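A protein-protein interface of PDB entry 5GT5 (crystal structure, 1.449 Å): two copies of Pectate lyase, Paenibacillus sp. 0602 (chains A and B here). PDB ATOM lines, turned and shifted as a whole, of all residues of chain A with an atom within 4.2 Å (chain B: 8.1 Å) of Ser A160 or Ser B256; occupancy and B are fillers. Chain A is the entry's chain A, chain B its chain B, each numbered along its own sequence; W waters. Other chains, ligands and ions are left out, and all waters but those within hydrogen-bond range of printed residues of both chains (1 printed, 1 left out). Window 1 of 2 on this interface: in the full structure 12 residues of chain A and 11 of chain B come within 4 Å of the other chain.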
ATOM      1  N   SER A 122      -8.761 -17.990 -12.517  1.00  0.00           N
ATOM      2  CA  SER A 122      -8.890 -16.569 -12.827  1.00  0.00           C
ATOM      3  C   SER A 122      -8.238 -16.241 -14.161  1.00  0.00           C
ATOM      4  O   SER A 122      -7.397 -16.991 -14.693  1.00  0.00           O
ATOM      5  CB  SER A 122      -8.247 -15.752 -11.715  1.00  0.00           C
ATOM      6  OG  SER A 122      -8.986 -15.875 -10.493  1.00  0.00           O
ATOM      7  N   SER A 123      -8.624 -15.109 -14.732  1.00  0.00           N
ATOM      8  CA  SER A 123      -8.058 -14.669 -15.997  1.00  0.00           C
ATOM      9  C   SER A 123      -7.781 -13.192 -15.944  1.00  0.00           C
ATOM     10  O   SER A 123      -8.480 -12.419 -15.259  1.00  0.00           O
ATOM     11  CB  SER A 123      -8.995 -14.982 -17.157  1.00  0.00           C
ATOM     12  OG  SER A 123     -10.276 -14.447 -16.884  1.00  0.00           O
ATOM     13  N   ASN A 124      -6.748 -12.799 -16.686  1.00  0.00           N
ATOM     14  CA  ASN A 124      -6.363 -11.409 -16.860  1.00  0.00           C
ATOM     15  C   ASN A 124      -6.160 -10.692 -15.521  1.00  0.00           C
ATOM     16  O   ASN A 124      -6.849  -9.732 -15.159  1.00  0.00           O
ATOM     17  CB  ASN A 124      -7.387 -10.717 -17.755  1.00  0.00           C
ATOM     18  CG  ASN A 124      -7.366 -11.287 -19.139  1.00  0.00           C
ATOM     19  OD1 ASN A 124      -6.302 -11.558 -19.683  1.00  0.00           O
ATOM     20  ND2 ASN A 124      -8.548 -11.605 -19.656  1.00  0.00           N
ATOM     21  N   SER A 159      -5.287 -20.947 -14.340  1.00  0.00           N
ATOM     22  CA  SER A 159      -5.535 -19.543 -14.679  1.00  0.00           C
ATOM     23  C   SER A 159      -4.955 -19.211 -16.058  1.00  0.00           C
ATOM     24  O   SER A 159      -4.228 -20.022 -16.671  1.00  0.00           O
ATOM     25  CB  SER A 159      -4.964 -18.636 -13.585  1.00  0.00           C
ATOM     26  OG  SER A 159      -5.727 -18.794 -12.375  1.00  0.00           O
ATOM     27  N   SER A 160      -5.300 -18.037 -16.579  1.00  0.00           N
ATOM     28  CA  SER A 160      -4.925 -17.634 -17.932  1.00  0.00           C
ATOM     29  C   SER A 160      -4.715 -16.143 -17.978  1.00  0.00           C
ATOM     30  O   SER A 160      -5.675 -15.398 -17.735  1.00  0.00           O
ATOM     31  CB  SER A 160      -6.051 -18.012 -18.904  1.00  0.00           C
ATOM     32  OG  SER A 160      -5.737 -17.657 -20.250  1.00  0.00           O
ATOM     33  N   GLY A 161      -3.496 -15.705 -18.305  1.00  0.00           N
ATOM     34  CA  GLY A 161      -3.197 -14.282 -18.391  1.00  0.00           C
ATOM     35  C   GLY A 161      -2.910 -13.673 -17.039  1.00  0.00           C
ATOM     36  O   GLY A 161      -3.812 -13.222 -16.344  1.00  0.00           O
ATOM     37  N   VAL A 162      -1.646 -13.707 -16.641  1.00  0.00           N
ATOM     38  CA  VAL A 162      -1.196 -13.170 -15.373  1.00  0.00           C
ATOM     39  C   VAL A 162       0.075 -12.392 -15.639  1.00  0.00           C
ATOM     40  O   VAL A 162       1.032 -12.956 -16.166  1.00  0.00           O
ATOM     41  CB  VAL A 162      -0.908 -14.282 -14.345  1.00  0.00           C
ATOM     42  CG1 VAL A 162      -0.448 -13.652 -13.021  1.00  0.00           C
ATOM     43  CG2 VAL A 162      -2.152 -15.170 -14.108  1.00  0.00           C
ATOM     44  N   SER A 184      -1.536 -20.794 -18.165  1.00  0.00           N
ATOM     45  CA  SER A 184      -0.871 -20.240 -19.356  1.00  0.00           C
ATOM     46  C   SER A 184      -0.932 -18.715 -19.374  1.00  0.00           C
ATOM     47  O   SER A 184      -1.701 -18.080 -18.629  1.00  0.00           O
ATOM     48  CB  SER A 184      -1.491 -20.787 -20.643  1.00  0.00           C
ATOM     49  OG  SER A 184      -2.861 -20.441 -20.711  1.00  0.00           O
ATOM     50  N   GLY B 182     -11.497 -11.079 -28.150  1.00  0.00           N
ATOM     51  CA  GLY B 182     -11.989 -10.394 -26.966  1.00  0.00           C
ATOM     52  C   GLY B 182     -13.266  -9.601 -27.127  1.00  0.00           C
ATOM     53  O   GLY B 182     -13.586  -8.817 -26.242  1.00  0.00           O
ATOM     54  N   THR B 252      -8.986 -18.951 -31.018  1.00  0.00           N
ATOM     55  CA  THR B 252      -7.641 -19.450 -30.759  1.00  0.00           C
ATOM     56  C   THR B 252      -7.563 -20.045 -29.360  1.00  0.00           C
ATOM     57  O   THR B 252      -7.983 -19.435 -28.393  1.00  0.00           O
ATOM     58  CB  THR B 252      -6.624 -18.323 -30.867  1.00  0.00           C
ATOM     59  OG1 THR B 252      -6.735 -17.710 -32.155  1.00  0.00           O
ATOM     60  CG2 THR B 252      -5.195 -18.880 -30.720  1.00  0.00           C
ATOM     61  N   SER B 253      -6.979 -21.226 -29.265  1.00  0.00           N
ATOM     62  CA  SER B 253      -6.919 -21.962 -28.013  1.00  0.00           C
ATOM     63  C   SER B 253      -6.093 -21.282 -26.932  1.00  0.00           C
ATOM     64  O   SER B 253      -4.978 -20.761 -27.186  1.00  0.00           O
ATOM     65  CB  SER B 253      -6.380 -23.366 -28.280  1.00  0.00           C
ATOM     66  OG  SER B 253      -6.409 -24.159 -27.123  1.00  0.00           O
ATOM     67  N   ASP B 254      -6.672 -21.261 -25.735  1.00  0.00           N
ATOM     68  CA  ASP B 254      -5.956 -20.871 -24.522  1.00  0.00           C
ATOM     69  C   ASP B 254      -5.375 -19.457 -24.571  1.00  0.00           C
ATOM     70  O   ASP B 254      -4.229 -19.233 -24.147  1.00  0.00           O
ATOM     71  CB  ASP B 254      -4.866 -21.899 -24.148  1.00  0.00           C
ATOM     72  CG  ASP B 254      -5.421 -23.251 -23.649  1.00  0.00           C
ATOM     73  OD1 ASP B 254      -6.556 -23.323 -23.082  1.00  0.00           O
ATOM     74  OD2 ASP B 254      -4.609 -24.241 -23.654  1.00  0.00           O
ATOM     75  N   GLU B 255      -6.094 -18.533 -25.195  1.00  0.00           N
ATOM     76  CA  GLU B 255      -5.757 -17.120 -25.136  1.00  0.00           C
ATOM     77  C   GLU B 255      -6.589 -16.436 -24.026  1.00  0.00           C
ATOM     78  O   GLU B 255      -7.810 -16.593 -24.000  1.00  0.00           O
ATOM     79  CB  GLU B 255      -6.070 -16.504 -26.491  1.00  0.00           C
ATOM     80  CG  GLU B 255      -5.117 -16.949 -27.588  1.00  0.00           C
ATOM     81  CD  GLU B 255      -3.652 -16.601 -27.309  1.00  0.00           C
ATOM     82  OE1 GLU B 255      -3.375 -15.509 -26.768  1.00  0.00           O
ATOM     83  OE2 GLU B 255      -2.774 -17.435 -27.631  1.00  0.00           O
ATOM     84  N   SER B 256      -5.977 -15.640 -23.145  1.00  0.00           N
ATOM     85  CA  SER B 256      -6.712 -15.011 -22.061  1.00  0.00           C
ATOM     86  C   SER B 256      -7.762 -14.000 -22.548  1.00  0.00           C
ATOM     87  O   SER B 256      -8.735 -13.769 -21.833  1.00  0.00           O
ATOM     88  CB  SER B 256      -5.782 -14.348 -21.009  1.00  0.00           C
ATOM     89  OG  SER B 256      -5.251 -13.117 -21.493  1.00  0.00           O
ATOM     90  N   ALA B 257      -7.581 -13.420 -23.745  1.00  0.00           N
ATOM     91  CA  ALA B 257      -8.589 -12.518 -24.297  1.00  0.00           C
ATOM     92  C   ALA B 257      -9.921 -13.228 -24.465  1.00  0.00           C
ATOM     93  O   ALA B 257     -10.983 -12.583 -24.460  1.00  0.00           O
ATOM     94  CB  ALA B 257      -8.140 -11.967 -25.632  1.00  0.00           C
ATOM     95  N   ASN B 258      -9.898 -14.555 -24.534  1.00  0.00           N
ATOM     96  CA  ASN B 258     -11.149 -15.286 -24.638  1.00  0.00           C
ATOM     97  C   ASN B 258     -12.045 -15.107 -23.416  1.00  0.00           C
ATOM     98  O   ASN B 258     -13.276 -15.215 -23.504  1.00  0.00           O
ATOM     99  CB  ASN B 258     -10.910 -16.772 -24.878  1.00  0.00           C
ATOM    100  CG  ASN B 258     -10.279 -17.066 -26.231  1.00  0.00           C
ATOM    101  OD1 ASN B 258     -10.417 -16.296 -27.198  1.00  0.00           O
ATOM    102  ND2 ASN B 258      -9.560 -18.194 -26.299  1.00  0.00           N
ATOM    103  N   ALA B 259     -11.419 -14.835 -22.270  1.00  0.00           N
ATOM    104  CA  ALA B 259     -12.171 -14.672 -21.049  1.00  0.00           C
ATOM    105  C   ALA B 259     -13.067 -13.442 -21.116  1.00  0.00           C
ATOM    106  O   ALA B 259     -14.093 -13.363 -20.407  1.00  0.00           O
ATOM    107  CB  ALA B 259     -11.231 -14.566 -19.866  1.00  0.00           C
ATOM    108  N   ASN B 260     -12.736 -12.523 -22.019  1.00  0.00           N
ATOM    109  CA  ASN B 260     -13.530 -11.309 -22.186  1.00  0.00           C
ATOM    110  C   ASN B 260     -14.706 -11.459 -23.133  1.00  0.00           C
ATOM    111  O   ASN B 260     -15.535 -10.558 -23.221  1.00  0.00           O
ATOM    112  CB  ASN B 260     -12.671 -10.156 -22.694  1.00  0.00           C
ATOM    113  CG  ASN B 260     -11.554  -9.804 -21.752  1.00  0.00           C
ATOM    114  OD1 ASN B 260     -11.734  -9.796 -20.534  1.00  0.00           O
ATOM    115  ND2 ASN B 260     -10.392  -9.487 -22.315  1.00  0.00           N
ATOM    116  N   LEU B 261     -14.772 -12.575 -23.844  1.00  0.00           N
ATOM    117  CA  LEU B 261     -15.928 -12.817 -24.731  1.00  0.00           C
ATOM    118  C   LEU B 261     -17.202 -12.929 -23.922  1.00  0.00           C
ATOM    119  O   LEU B 261     -17.275 -13.673 -22.935  1.00  0.00           O
ATOM    120  CB  LEU B 261     -15.723 -14.109 -25.530  1.00  0.00           C
ATOM    121  CG  LEU B 261     -14.499 -14.096 -26.437  1.00  0.00           C
ATOM    122  CD1 LEU B 261     -14.094 -15.521 -26.731  1.00  0.00           C
ATOM    123  CD2 LEU B 261     -14.746 -13.295 -27.717  1.00  0.00           C
ATOM    124  N   ARG B 281     -14.860 -20.625 -26.100  1.00  0.00           N
ATOM    125  CA  ARG B 281     -13.647 -20.757 -25.310  1.00  0.00           C
ATOM    126  C   ARG B 281     -13.631 -19.634 -24.288  1.00  0.00           C
ATOM    127  O   ARG B 281     -13.798 -18.459 -24.647  1.00  0.00           O
ATOM    128  CB  ARG B 281     -12.423 -20.574 -26.194  1.00  0.00           C
ATOM    129  CG  ARG B 281     -12.118 -21.723 -27.127  1.00  0.00           C
ATOM    130  CD  ARG B 281     -10.858 -21.424 -27.924  1.00  0.00           C
ATOM    131  NE  ARG B 281     -10.354 -22.646 -28.555  1.00  0.00           N
ATOM    132  CZ  ARG B 281     -10.615 -23.035 -29.805  1.00  0.00           C
ATOM    133  NH1 ARG B 281     -11.313 -22.263 -30.617  1.00  0.00           N
ATOM    134  NH2 ARG B 281     -10.093 -24.175 -30.277  1.00  0.00           N
ATOM    135  N   GLY B 282     -13.417 -19.988 -23.025  1.00  0.00           N
ATOM    136  CA  GLY B 282     -12.988 -19.029 -22.001  1.00  0.00           C
ATOM    137  C   GLY B 282     -13.990 -18.049 -21.426  1.00  0.00           C
ATOM    138  O   GLY B 282     -13.936 -17.761 -20.238  1.00  0.00           O
ATOM    139  N   GLY B 283     -14.885 -17.525 -22.255  1.00  0.00           N
ATOM    140  CA  GLY B 283     -15.740 -16.422 -21.805  1.00  0.00           C
ATOM    141  C   GLY B 283     -17.056 -16.852 -21.190  1.00  0.00           C
ATOM    142  O   GLY B 283     -17.136 -17.836 -20.466  1.00  0.00           O
ATOM    143  N   GLU B 330     -12.323 -24.837 -22.409  1.00  0.00           N
ATOM    144  CA  GLU B 330     -11.239 -23.972 -21.927  1.00  0.00           C
ATOM    145  C   GLU B 330     -11.722 -22.988 -20.878  1.00  0.00           C
ATOM    146  O   GLU B 330     -11.509 -21.780 -20.937  1.00  0.00           O
ATOM    147  CB  GLU B 330     -10.571 -23.259 -23.119  1.00  0.00           C
ATOM    148  CG  GLU B 330     -10.051 -24.257 -24.171  1.00  0.00           C
ATOM    149  CD  GLU B 330      -9.441 -23.572 -25.364  1.00  0.00           C
ATOM    150  OE1 GLU B 330      -9.152 -22.376 -25.272  1.00  0.00           O
ATOM    151  OE2 GLU B 330      -9.250 -24.269 -26.387  1.00  0.00           O
ATOM    152  N   SER B 331     -12.413 -23.548 -19.895  1.00  0.00           N
ATOM    153  CA  SER B 331     -12.873 -22.806 -18.719  1.00  0.00           C
ATOM    154  C   SER B 331     -13.955 -21.788 -19.007  1.00  0.00           C
ATOM    155  O   SER B 331     -14.280 -20.991 -18.152  1.00  0.00           O
ATOM    156  CB  SER B 331     -11.704 -22.169 -17.972  1.00  0.00           C
ATOM    157  OG  SER B 331     -10.773 -23.182 -17.569  1.00  0.00           O
ATOM    158  N   THR B 359      -7.566 -28.606 -18.629  1.00  0.00           N
ATOM    159  CA  THR B 359      -7.339 -27.279 -19.184  1.00  0.00           C
ATOM    160  C   THR B 359      -8.283 -27.047 -20.378  1.00  0.00           C
ATOM    161  O   THR B 359      -8.716 -25.936 -20.643  1.00  0.00           O
ATOM    162  CB  THR B 359      -5.890 -27.095 -19.643  1.00  0.00           C
ATOM    163  OG1 THR B 359      -4.975 -27.654 -18.672  1.00  0.00           O
ATOM    164  CG2 THR B 359      -5.572 -25.628 -19.875  1.00  0.00           C
HETATM  165  O   HOH W   1      -3.508 -18.072 -21.724  1.00  0.00           O
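The side-chain amide oxygen (OD1) of Asn A124 is in hydrogen-bond range of the side-chain hydroxyl (OG) of Ser B256, at 2.6 Å.
N of Ser A160 sits at hydrogen-bond distance from O of Ser A122 (3.0 Å). The backbone NH (N) of Asn A124 is in hydrogen-bond range of the backbone carbonyl oxygen (O) of Ser A160, at 3.0 Å. O of Gly A161 is in hydrogen-bond range of N of Asn A124, 3.0 Å away. The backbone carbonyl oxygen (O) of Ser A159 sits at hydrogen-bond distance from the backbone NH (N) of Ser A184. O of Ser A184 lies within hydrogen-bond range of N of Gly A161, at 3.0 Å. OE1 of Glu B330 lies within hydrogen-bond range of N of Asp B254, 2.8 Å away.
Among the printed residues, merely in contact across the chains: Ser A123 with Ala B259 (3.1 Å), Ser A160 with Ser B256 (3.4 Å), Gly A161 with Ser B256 (3.7 Å), Asn A124 with Asn B260 (3.8 Å) and Ser A184 with Asp B254 (3.9 Å).
Printed residues of chain B within 4 Å of Ser A123: Ala B259 (3.1 Å). Printed residues of chain B within 4 Å of Asn A124: Ser B256 and Asn B260. Of chain B, only Ser B256 comes within 4 Å of Ser A160. Gly A161 touches just one residue of chain B: Ser B256 (3.7 Å). Gly B182 touches none of the printed residues of chain A. Printed residues of chain A within 4 Å of Asp B254: Ser A184 (3.9 Å). Of the printed residues of chain A, Ser B256 touches Asn A124 (2.6 Å), Ser A160 (3.4 Å) and Gly A161 (3.7 Å). Printed residues of chain A within 4 Å of Asn B260: Asn A124. Glu B330 touches none of the printed residues of chain A. The nearest printed residue of chain A that does not touch Ser B256 is Ser A123 (4.8 Å).
Hydrophobic or aromatic side chains of chain B within 4 Å of the printed part of chain A: Ala B259. Along chain B the printed residues that touch a printed residue of chain A span positions 254 to 260. Of the 8 printed residues of chain A, 5 touch a printed residue of chain B. Among the printed residues, 6 pairs touch across the chains. Among the printed residues, no Asp or Glu carboxylate lies within 4 Å of a Lys or Arg side-chain nitrogen of the other chain.
No position is printed for both chains.
Water W1 lies within hydrogen-bond range of the side-chain hydroxyl of Ser A184 (2.7 Å), the side-chain hydroxyl of Ser A160 (2.7 Å) and the backbone carbonyl oxygen of Asp B254 (2.8 Å).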
